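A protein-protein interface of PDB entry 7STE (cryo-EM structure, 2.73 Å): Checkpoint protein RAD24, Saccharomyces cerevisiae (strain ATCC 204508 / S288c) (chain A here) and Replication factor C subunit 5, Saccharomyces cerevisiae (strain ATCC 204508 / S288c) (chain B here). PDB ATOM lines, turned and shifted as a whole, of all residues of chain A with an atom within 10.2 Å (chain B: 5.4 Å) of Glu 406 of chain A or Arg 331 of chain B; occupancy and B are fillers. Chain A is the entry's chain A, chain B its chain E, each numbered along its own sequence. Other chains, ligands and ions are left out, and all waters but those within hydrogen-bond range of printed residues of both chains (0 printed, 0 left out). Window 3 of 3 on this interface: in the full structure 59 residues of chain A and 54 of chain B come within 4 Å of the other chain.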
ATOM      1  N   LYS A 377      30.006 -10.937 -10.886  1.00  0.00           N
ATOM      2  CA  LYS A 377      30.251 -10.209 -12.126  1.00  0.00           C
ATOM      3  C   LYS A 377      30.730  -8.795 -11.834  1.00  0.00           C
ATOM      4  O   LYS A 377      31.772  -8.365 -12.344  1.00  0.00           O
ATOM      5  CB  LYS A 377      28.988 -10.182 -12.986  1.00  0.00           C
ATOM      6  CG  LYS A 377      28.854 -11.370 -13.925  1.00  0.00           C
ATOM      7  CD  LYS A 377      27.406 -11.624 -14.318  1.00  0.00           C
ATOM      8  CE  LYS A 377      26.742 -10.377 -14.887  1.00  0.00           C
ATOM      9  NZ  LYS A 377      27.509  -9.800 -16.027  1.00  0.00           N
ATOM     10  N   SER A 398      37.477  -3.178 -23.513  1.00  0.00           N
ATOM     11  CA  SER A 398      36.201  -3.034 -24.206  1.00  0.00           C
ATOM     12  C   SER A 398      35.548  -4.389 -24.434  1.00  0.00           C
ATOM     13  O   SER A 398      34.340  -4.546 -24.226  1.00  0.00           O
ATOM     14  CB  SER A 398      36.407  -2.309 -25.535  1.00  0.00           C
ATOM     15  OG  SER A 398      35.227  -2.332 -26.318  1.00  0.00           O
ATOM     16  N   SER A 399      36.331  -5.382 -24.862  1.00  0.00           N
ATOM     17  CA  SER A 399      35.780  -6.716 -25.074  1.00  0.00           C
ATOM     18  C   SER A 399      35.264  -7.309 -23.769  1.00  0.00           C
ATOM     19  O   SER A 399      34.183  -7.912 -23.735  1.00  0.00           O
ATOM     20  CB  SER A 399      36.838  -7.627 -25.694  1.00  0.00           C
ATOM     21  OG  SER A 399      37.087  -7.275 -27.043  1.00  0.00           O
ATOM     22  N   ILE A 400      36.021  -7.146 -22.683  1.00  0.00           N
ATOM     23  CA  ILE A 400      35.605  -7.696 -21.396  1.00  0.00           C
ATOM     24  C   ILE A 400      34.298  -7.054 -20.946  1.00  0.00           C
ATOM     25  O   ILE A 400      33.377  -7.737 -20.484  1.00  0.00           O
ATOM     26  CB  ILE A 400      36.717  -7.505 -20.347  1.00  0.00           C
ATOM     27  CG1 ILE A 400      37.911  -8.407 -20.669  1.00  0.00           C
ATOM     28  CG2 ILE A 400      36.191  -7.802 -18.950  1.00  0.00           C
ATOM     29  CD1 ILE A 400      39.214  -7.932 -20.062  1.00  0.00           C
ATOM     30  N   VAL A 401      34.197  -5.730 -21.077  1.00  0.00           N
ATOM     31  CA  VAL A 401      32.987  -5.037 -20.648  1.00  0.00           C
ATOM     32  C   VAL A 401      31.803  -5.430 -21.523  1.00  0.00           C
ATOM     33  O   VAL A 401      30.682  -5.599 -21.029  1.00  0.00           O
ATOM     34  CB  VAL A 401      33.209  -3.515 -20.652  1.00  0.00           C
ATOM     35  CG1 VAL A 401      31.912  -2.795 -20.316  1.00  0.00           C
ATOM     36  CG2 VAL A 401      34.297  -3.135 -19.660  1.00  0.00           C
ATOM     37  N   ASP A 402      32.021  -5.561 -22.833  1.00  0.00           N
ATOM     38  CA  ASP A 402      30.935  -5.972 -23.715  1.00  0.00           C
ATOM     39  C   ASP A 402      30.438  -7.364 -23.349  1.00  0.00           C
ATOM     40  O   ASP A 402      29.227  -7.613 -23.309  1.00  0.00           O
ATOM     41  CB  ASP A 402      31.397  -5.927 -25.171  1.00  0.00           C
ATOM     42  CG  ASP A 402      30.240  -5.942 -26.150  1.00  0.00           C
ATOM     43  OD1 ASP A 402      29.177  -5.373 -25.826  1.00  0.00           O
ATOM     44  OD2 ASP A 402      30.394  -6.521 -27.245  1.00  0.00           O
ATOM     45  N   CYS A 403      31.363  -8.286 -23.067  1.00  0.00           N
ATOM     46  CA  CYS A 403      30.953  -9.616 -22.634  1.00  0.00           C
ATOM     47  C   CYS A 403      30.194  -9.564 -21.317  1.00  0.00           C
ATOM     48  O   CYS A 403      29.214 -10.293 -21.133  1.00  0.00           O
ATOM     49  CB  CYS A 403      32.160 -10.532 -22.478  1.00  0.00           C
ATOM     50  SG  CYS A 403      31.684 -12.096 -21.723  1.00  0.00           S
ATOM     51  N   LEU A 404      30.654  -8.741 -20.375  1.00  0.00           N
ATOM     52  CA  LEU A 404      29.965  -8.643 -19.094  1.00  0.00           C
ATOM     53  C   LEU A 404      28.549  -8.115 -19.281  1.00  0.00           C
ATOM     54  O   LEU A 404      27.607  -8.600 -18.646  1.00  0.00           O
ATOM     55  CB  LEU A 404      30.757  -7.750 -18.139  1.00  0.00           C
ATOM     56  CG  LEU A 404      32.040  -8.358 -17.558  1.00  0.00           C
ATOM     57  CD1 LEU A 404      32.740  -7.360 -16.651  1.00  0.00           C
ATOM     58  CD2 LEU A 404      31.753  -9.650 -16.806  1.00  0.00           C
ATOM     59  N   SER A 405      28.381  -7.125 -20.159  1.00  0.00           N
ATOM     60  CA  SER A 405      27.045  -6.614 -20.452  1.00  0.00           C
ATOM     61  C   SER A 405      26.169  -7.691 -21.081  1.00  0.00           C
ATOM     62  O   SER A 405      24.998  -7.847 -20.709  1.00  0.00           O
ATOM     63  CB  SER A 405      27.145  -5.399 -21.373  1.00  0.00           C
ATOM     64  OG  SER A 405      25.906  -5.140 -22.007  1.00  0.00           O
ATOM     65  N   GLU A 406      26.718  -8.449 -22.033  1.00  0.00           N
ATOM     66  CA  GLU A 406      25.943  -9.519 -22.654  1.00  0.00           C
ATOM     67  C   GLU A 406      25.528 -10.564 -21.625  1.00  0.00           C
ATOM     68  O   GLU A 406      24.386 -11.037 -21.633  1.00  0.00           O
ATOM     69  CB  GLU A 406      26.746 -10.168 -23.781  1.00  0.00           C
ATOM     70  CG  GLU A 406      26.991  -9.258 -24.972  1.00  0.00           C
ATOM     71  CD  GLU A 406      27.806  -9.926 -26.060  1.00  0.00           C
ATOM     72  OE1 GLU A 406      28.287 -11.057 -25.835  1.00  0.00           O
ATOM     73  OE2 GLU A 406      27.966  -9.322 -27.142  1.00  0.00           O
ATOM     74  N   CYS A 407      26.445 -10.936 -20.729  1.00  0.00           N
ATOM     75  CA  CYS A 407      26.115 -11.898 -19.683  1.00  0.00           C
ATOM     76  C   CYS A 407      25.042 -11.348 -18.754  1.00  0.00           C
ATOM     77  O   CYS A 407      24.147 -12.083 -18.323  1.00  0.00           O
ATOM     78  CB  CYS A 407      27.372 -12.265 -18.895  1.00  0.00           C
ATOM     79  SG  CYS A 407      28.584 -13.223 -19.835  1.00  0.00           S
ATOM     80  N   ASP A 408      25.119 -10.056 -18.430  1.00  0.00           N
ATOM     81  CA  ASP A 408      24.084  -9.441 -17.607  1.00  0.00           C
ATOM     82  C   ASP A 408      22.727  -9.517 -18.295  1.00  0.00           C
ATOM     83  O   ASP A 408      21.707  -9.778 -17.647  1.00  0.00           O
ATOM     84  CB  ASP A 408      24.450  -7.989 -17.302  1.00  0.00           C
ATOM     85  CG  ASP A 408      23.392  -7.284 -16.477  1.00  0.00           C
ATOM     86  OD1 ASP A 408      23.224  -7.640 -15.292  1.00  0.00           O
ATOM     87  OD2 ASP A 408      22.728  -6.372 -17.013  1.00  0.00           O
ATOM     88  N   ASN A 409      22.695  -9.290 -19.610  1.00  0.00           N
ATOM     89  CA  ASN A 409      21.441  -9.397 -20.345  1.00  0.00           C
ATOM     90  C   ASN A 409      20.885 -10.816 -20.338  1.00  0.00           C
ATOM     91  O   ASN A 409      19.677 -10.995 -20.527  1.00  0.00           O
ATOM     92  CB  ASN A 409      21.632  -8.928 -21.786  1.00  0.00           C
ATOM     93  CG  ASN A 409      21.475  -7.429 -21.936  1.00  0.00           C
ATOM     94  OD1 ASN A 409      21.430  -6.694 -20.950  1.00  0.00           O
ATOM     95  ND2 ASN A 409      21.383  -6.967 -23.176  1.00  0.00           N
ATOM     96  N   MET A 410      21.732 -11.825 -20.125  1.00  0.00           N
ATOM     97  CA  MET A 410      21.263 -13.206 -20.107  1.00  0.00           C
ATOM     98  C   MET A 410      20.398 -13.518 -18.893  1.00  0.00           C
ATOM     99  O   MET A 410      19.773 -14.583 -18.858  1.00  0.00           O
ATOM    100  CB  MET A 410      22.457 -14.162 -20.156  1.00  0.00           C
ATOM    101  CG  MET A 410      23.140 -14.210 -21.514  1.00  0.00           C
ATOM    102  SD  MET A 410      24.663 -15.173 -21.510  1.00  0.00           S
ATOM    103  CE  MET A 410      24.006 -16.833 -21.379  1.00  0.00           C
ATOM    104  N   ASN A 411      20.347 -12.624 -17.906  1.00  0.00           N
ATOM    105  CA  ASN A 411      19.453 -12.754 -16.756  1.00  0.00           C
ATOM    106  C   ASN A 411      19.767 -14.014 -15.946  1.00  0.00           C
ATOM    107  O   ASN A 411      18.926 -14.896 -15.757  1.00  0.00           O
ATOM    108  CB  ASN A 411      17.989 -12.739 -17.208  1.00  0.00           C
ATOM    109  CG  ASN A 411      17.581 -11.409 -17.815  1.00  0.00           C
ATOM    110  OD1 ASN A 411      17.905 -10.347 -17.283  1.00  0.00           O
ATOM    111  ND2 ASN A 411      16.869 -11.462 -18.934  1.00  0.00           N
ATOM    112  N   GLY A 412      21.007 -14.081 -15.468  1.00  0.00           N
ATOM    113  CA  GLY A 412      21.408 -15.100 -14.518  1.00  0.00           C
ATOM    114  C   GLY A 412      21.227 -16.527 -14.993  1.00  0.00           C
ATOM    115  O   GLY A 412      20.774 -17.383 -14.227  1.00  0.00           O
ATOM    116  N   LEU A 413      21.576 -16.801 -16.254  1.00  0.00           N
ATOM    117  CA  LEU A 413      21.536 -18.178 -16.720  1.00  0.00           C
ATOM    118  C   LEU A 413      22.844 -18.888 -16.383  1.00  0.00           C
ATOM    119  O   LEU A 413      23.886 -18.243 -16.229  1.00  0.00           O
ATOM    120  CB  LEU A 413      21.303 -18.227 -18.229  1.00  0.00           C
ATOM    121  CG  LEU A 413      19.864 -18.062 -18.726  1.00  0.00           C
ATOM    122  CD1 LEU A 413      19.817 -18.190 -20.240  1.00  0.00           C
ATOM    123  CD2 LEU A 413      18.925 -19.073 -18.082  1.00  0.00           C
ATOM    124  N   GLU A 415      24.756 -20.536 -18.282  1.00  0.00           N
ATOM    125  CA  GLU A 415      25.739 -20.353 -19.343  1.00  0.00           C
ATOM    126  C   GLU A 415      26.380 -18.971 -19.289  1.00  0.00           C
ATOM    127  O   GLU A 415      27.506 -18.795 -19.769  1.00  0.00           O
ATOM    128  CB  GLU A 415      25.086 -20.574 -20.708  1.00  0.00           C
ATOM    129  CG  GLU A 415      24.472 -21.957 -20.891  1.00  0.00           C
ATOM    130  CD  GLU A 415      23.022 -22.025 -20.452  1.00  0.00           C
ATOM    131  OE1 GLU A 415      22.519 -21.034 -19.881  1.00  0.00           O
ATOM    132  OE2 GLU A 415      22.380 -23.072 -20.678  1.00  0.00           O
ATOM    133  N   SER A 416      25.685 -17.984 -18.720  1.00  0.00           N
ATOM    134  CA  SER A 416      26.205 -16.620 -18.710  1.00  0.00           C
ATOM    135  C   SER A 416      27.497 -16.528 -17.906  1.00  0.00           C
ATOM    136  O   SER A 416      28.484 -15.939 -18.361  1.00  0.00           O
ATOM    137  CB  SER A 416      25.152 -15.664 -18.148  1.00  0.00           C
ATOM    138  OG  SER A 416      24.816 -16.004 -16.815  1.00  0.00           O
ATOM    139  N   ASN A 417      27.502 -17.092 -16.697  1.00  0.00           N
ATOM    140  CA  ASN A 417      28.705 -17.049 -15.870  1.00  0.00           C
ATOM    141  C   ASN A 417      29.847 -17.812 -16.529  1.00  0.00           C
ATOM    142  O   ASN A 417      30.994 -17.345 -16.540  1.00  0.00           O
ATOM    143  CB  ASN A 417      28.408 -17.619 -14.484  1.00  0.00           C
ATOM    144  CG  ASN A 417      27.141 -17.046 -13.875  1.00  0.00           C
ATOM    145  OD1 ASN A 417      26.258 -17.786 -13.442  1.00  0.00           O
ATOM    146  ND2 ASN A 417      27.046 -15.722 -13.842  1.00  0.00           N
ATOM    147  N   TYR A 419      30.364 -18.309 -19.740  1.00  0.00           N
ATOM    148  CA  TYR A 419      30.859 -17.537 -20.874  1.00  0.00           C
ATOM    149  C   TYR A 419      31.677 -16.339 -20.408  1.00  0.00           C
ATOM    150  O   TYR A 419      32.751 -16.054 -20.955  1.00  0.00           O
ATOM    151  CB  TYR A 419      29.674 -17.082 -21.726  1.00  0.00           C
ATOM    152  CG  TYR A 419      30.008 -16.019 -22.742  1.00  0.00           C
ATOM    153  CD1 TYR A 419      31.112 -16.149 -23.570  1.00  0.00           C
ATOM    154  CD2 TYR A 419      29.228 -14.876 -22.859  1.00  0.00           C
ATOM    155  CE1 TYR A 419      31.420 -15.181 -24.504  1.00  0.00           C
ATOM    156  CE2 TYR A 419      29.533 -13.895 -23.788  1.00  0.00           C
ATOM    157  CZ  TYR A 419      30.636 -14.053 -24.605  1.00  0.00           C
ATOM    158  OH  TYR A 419      30.958 -13.092 -25.537  1.00  0.00           O
ATOM    159  N   GLY A 420      31.180 -15.616 -19.402  1.00  0.00           N
ATOM    160  CA  GLY A 420      31.897 -14.442 -18.929  1.00  0.00           C
ATOM    161  C   GLY A 420      33.257 -14.788 -18.357  1.00  0.00           C
ATOM    162  O   GLY A 420      34.266 -14.155 -18.685  1.00  0.00           O
ATOM    163  N   GLU A 423      35.645 -15.855 -21.235  1.00  0.00           N
ATOM    164  CA  GLU A 423      36.183 -14.654 -21.877  1.00  0.00           C
ATOM    165  C   GLU A 423      37.252 -13.982 -21.032  1.00  0.00           C
ATOM    166  O   GLU A 423      38.307 -13.611 -21.551  1.00  0.00           O
ATOM    167  CB  GLU A 423      35.087 -13.634 -22.189  1.00  0.00           C
ATOM    168  CG  GLU A 423      34.079 -14.007 -23.242  1.00  0.00           C
ATOM    169  CD  GLU A 423      34.707 -14.096 -24.613  1.00  0.00           C
ATOM    170  OE1 GLU A 423      35.674 -13.347 -24.866  1.00  0.00           O
ATOM    171  OE2 GLU A 423      34.206 -14.857 -25.460  1.00  0.00           O
ATOM    172  N   SER B 326      22.715   3.479 -29.541  1.00  0.00           N
ATOM    173  CA  SER B 326      21.464   2.752 -29.734  1.00  0.00           C
ATOM    174  C   SER B 326      21.565   1.332 -29.186  1.00  0.00           C
ATOM    175  O   SER B 326      20.663   0.854 -28.481  1.00  0.00           O
ATOM    176  CB  SER B 326      21.099   2.731 -31.219  1.00  0.00           C
ATOM    177  OG  SER B 326      20.109   1.754 -31.488  1.00  0.00           O
ATOM    178  N   VAL B 327      22.668   0.644 -29.492  1.00  0.00           N
ATOM    179  CA  VAL B 327      22.823  -0.740 -29.052  1.00  0.00           C
ATOM    180  C   VAL B 327      22.830  -0.814 -27.531  1.00  0.00           C
ATOM    181  O   VAL B 327      22.165  -1.664 -26.925  1.00  0.00           O
ATOM    182  CB  VAL B 327      24.101  -1.353 -29.655  1.00  0.00           C
ATOM    183  CG1 VAL B 327      24.484  -2.631 -28.920  1.00  0.00           C
ATOM    184  CG2 VAL B 327      23.909  -1.620 -31.139  1.00  0.00           C
ATOM    185  N   PHE B 328      23.574   0.084 -26.885  1.00  0.00           N
ATOM    186  CA  PHE B 328      23.684   0.033 -25.434  1.00  0.00           C
ATOM    187  C   PHE B 328      22.427   0.552 -24.748  1.00  0.00           C
ATOM    188  O   PHE B 328      22.133   0.140 -23.624  1.00  0.00           O
ATOM    189  CB  PHE B 328      24.919   0.808 -24.981  1.00  0.00           C
ATOM    190  CG  PHE B 328      26.188   0.011 -25.075  1.00  0.00           C
ATOM    191  CD1 PHE B 328      26.492  -0.947 -24.123  1.00  0.00           C
ATOM    192  CD2 PHE B 328      27.066   0.200 -26.129  1.00  0.00           C
ATOM    193  CE1 PHE B 328      27.653  -1.690 -24.212  1.00  0.00           C
ATOM    194  CE2 PHE B 328      28.230  -0.540 -26.223  1.00  0.00           C
ATOM    195  CZ  PHE B 328      28.522  -1.486 -25.264  1.00  0.00           C
ATOM    196  N   ASP B 329      21.661   1.431 -25.399  1.00  0.00           N
ATOM    197  CA  ASP B 329      20.347   1.783 -24.874  1.00  0.00           C
ATOM    198  C   ASP B 329      19.418   0.577 -24.893  1.00  0.00           C
ATOM    199  O   ASP B 329      18.688   0.329 -23.924  1.00  0.00           O
ATOM    200  CB  ASP B 329      19.753   2.936 -25.682  1.00  0.00           C
ATOM    201  CG  ASP B 329      18.528   3.540 -25.025  1.00  0.00           C
ATOM    202  OD1 ASP B 329      18.610   3.902 -23.832  1.00  0.00           O
ATOM    203  OD2 ASP B 329      17.486   3.655 -25.700  1.00  0.00           O
ATOM    204  N   GLU B 330      19.440  -0.193 -25.984  1.00  0.00           N
ATOM    205  CA  GLU B 330      18.667  -1.430 -26.015  1.00  0.00           C
ATOM    206  C   GLU B 330      19.128  -2.383 -24.920  1.00  0.00           C
ATOM    207  O   GLU B 330      18.306  -3.031 -24.261  1.00  0.00           O
ATOM    208  CB  GLU B 330      18.784  -2.096 -27.385  1.00  0.00           C
ATOM    209  CG  GLU B 330      17.714  -3.149 -27.646  1.00  0.00           C
ATOM    210  CD  GLU B 330      18.028  -4.023 -28.845  1.00  0.00           C
ATOM    211  OE1 GLU B 330      19.180  -3.987 -29.328  1.00  0.00           O
ATOM    212  OE2 GLU B 330      17.121  -4.748 -29.304  1.00  0.00           O
ATOM    213  N   ARG B 331      20.443  -2.482 -24.712  1.00  0.00           N
ATOM    214  CA  ARG B 331      20.961  -3.334 -23.645  1.00  0.00           C
ATOM    215  C   ARG B 331      20.469  -2.865 -22.279  1.00  0.00           C
ATOM    216  O   ARG B 331      20.088  -3.682 -21.432  1.00  0.00           O
ATOM    217  CB  ARG B 331      22.489  -3.352 -23.684  1.00  0.00           C
ATOM    218  CG  ARG B 331      23.082  -3.833 -25.003  1.00  0.00           C
ATOM    219  CD  ARG B 331      23.538  -5.282 -24.926  1.00  0.00           C
ATOM    220  NE  ARG B 331      24.407  -5.644 -26.041  1.00  0.00           N
ATOM    221  CZ  ARG B 331      25.733  -5.673 -25.992  1.00  0.00           C
ATOM    222  NH1 ARG B 331      26.395  -5.350 -24.891  1.00  0.00           N
ATOM    223  NH2 ARG B 331      26.414  -6.033 -27.076  1.00  0.00           N
ATOM    224  N   LEU B 332      20.472  -1.550 -22.048  1.00  0.00           N
ATOM    225  CA  LEU B 332      19.963  -1.006 -20.793  1.00  0.00           C
ATOM    226  C   LEU B 332      18.496  -1.355 -20.601  1.00  0.00           C
ATOM    227  O   LEU B 332      18.068  -1.691 -19.490  1.00  0.00           O
ATOM    228  CB  LEU B 332      20.149   0.512 -20.765  1.00  0.00           C
ATOM    229  CG  LEU B 332      21.559   1.052 -20.528  1.00  0.00           C
ATOM    230  CD1 LEU B 332      21.633   2.519 -20.919  1.00  0.00           C
ATOM    231  CD2 LEU B 332      21.953   0.878 -19.072  1.00  0.00           C
ATOM    232  N   SER B 333      17.705  -1.279 -21.673  1.00  0.00           N
ATOM    233  CA  SER B 333      16.283  -1.579 -21.556  1.00  0.00           C
ATOM    234  C   SER B 333      16.058  -3.008 -21.076  1.00  0.00           C
ATOM    235  O   SER B 333      15.185  -3.261 -20.239  1.00  0.00           O
ATOM    236  CB  SER B 333      15.588  -1.349 -22.897  1.00  0.00           C
ATOM    237  OG  SER B 333      14.206  -1.646 -22.813  1.00  0.00           O
ATOM    238  N   LEU B 334      16.838  -3.957 -21.594  1.00  0.00           N
ATOM    239  CA  LEU B 334      16.693  -5.366 -21.256  1.00  0.00           C
ATOM    240  C   LEU B 334      17.660  -5.817 -20.166  1.00  0.00           C
ATOM    241  O   LEU B 334      17.686  -7.006 -19.834  1.00  0.00           O
ATOM    242  CB  LEU B 334      16.891  -6.224 -22.506  1.00  0.00           C
ATOM    243  CG  LEU B 334      15.933  -5.946 -23.666  1.00  0.00           C
ATOM    244  CD1 LEU B 334      16.408  -6.645 -24.929  1.00  0.00           C
ATOM    245  CD2 LEU B 334      14.518  -6.375 -23.312  1.00  0.00           C
ATOM    246  N   GLY B 335      18.449  -4.902 -19.601  1.00  0.00           N
ATOM    247  CA  GLY B 335      19.438  -5.246 -18.605  1.00  0.00           C
ATOM    248  C   GLY B 335      18.940  -5.036 -17.180  1.00  0.00           C
ATOM    249  O   GLY B 335      17.812  -4.621 -16.929  1.00  0.00           O
ATOM    250  N   HIS B 341      26.521  -1.527 -19.132  1.00  0.00           N
ATOM    251  CA  HIS B 341      26.220  -0.988 -20.453  1.00  0.00           C
ATOM    252  C   HIS B 341      26.835   0.390 -20.671  1.00  0.00           C
ATOM    253  O   HIS B 341      27.349   0.671 -21.758  1.00  0.00           O
ATOM    254  CB  HIS B 341      24.703  -0.930 -20.654  1.00  0.00           C
ATOM    255  CG  HIS B 341      23.981  -2.132 -20.130  1.00  0.00           C
ATOM    256  ND1 HIS B 341      23.980  -3.343 -20.788  1.00  0.00           N
ATOM    257  CD2 HIS B 341      23.253  -2.315 -19.003  1.00  0.00           C
ATOM    258  CE1 HIS B 341      23.273  -4.217 -20.093  1.00  0.00           C
ATOM    259  NE2 HIS B 341      22.821  -3.619 -19.007  1.00  0.00           N
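The guanidinium group (NH1) of Arg 331 of chain B lies within salt-bridge range of the side-chain carboxylate (OD1) of Asp 402 of chain A (2.9 Å).
NH1 of Arg 331 of chain B sits at hydrogen-bond distance from OG of Ser 405 of chain A, 2.9 Å away.
The guanidinium group (NH2) of Arg 331 of chain B is in salt-bridge range of the side-chain carboxylate (OE2) of Glu 406 of chain A, 3.6 Å away.
The backbone carbonyl oxygen (O) of Arg 331 of chain B lies close to the side-chain amide oxygen (OD1) of Asn 409 of chain A (3.3 Å).
A ring nitrogen (ND1) of His 341 of chain B sits at hydrogen-bond distance from the side-chain hydroxyl of Ser 405 of chain A, at 2.9 Å.
A ring nitrogen (NE2) of His 341 of chain B lies within hydrogen-bond range of the side-chain carboxylate (OD2) of Asp 408 of chain A.
OE1 of Glu 406 of chain A sits at hydrogen-bond distance from OH of Tyr 419 of chain A, 3.4 Å away.
The side-chain amide nitrogen (ND2) of Asn 411 of chain A lies within hydrogen-bond range of the backbone carbonyl oxygen (O) of Asn 409 of chain A (3.3 Å).
Among the printed residues, pairs that only touch across the chains: Asn 409 of chain A with His 341 of chain B, Asn 409 of chain A with Gly 335 of chain B, Asp 408 of chain A with Gly 335 of chain B, Asn 409 of chain A with Leu 334 of chain B and Asp 402 of chain A with Phe 328 of chain B.
Glu 406 of chain A touches just one residue of chain B: Arg 331 (3.6 Å).
Printed residues of chain A within 4 Å of Arg 331 of chain B: Asp 402 (2.9 Å), Ser 405 (2.9 Å), Glu 406 (3.6 Å) and Asn 409 (3.2 Å).
No residue of chain A comes within 4 Å of Glu 330 of chain B.
No residue of chain A comes within 4 Å of Leu 332 of chain B.
Of chain A, only Asp 408 and Asn 409 come within 4 Å of Gly 335 of chain B.
Of the printed residues of chain A, Phe 328 of chain B touches Asp 402 (3.98 Å).
Of the printed residues of chain A, Leu 334 of chain B touches Asn 409.
Tyr 419 of chain A touches none of the printed residues of chain B.
Ser 333 of chain B touches none of the printed residues of chain A.
The nearest residue of chain A that does not touch Arg 331 of chain B is Val 401 of chain A (5.8 Å).
The nearest printed residue of chain B that does not touch Asn 409 of chain A is Glu 330 of chain B (5.1 Å).
Hydrophobic or aromatic side chains of chain B within 4 Å of the printed part of chain A: Phe 328 and His 341.
Among the printed residues, 11 pairs touch across the chains.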
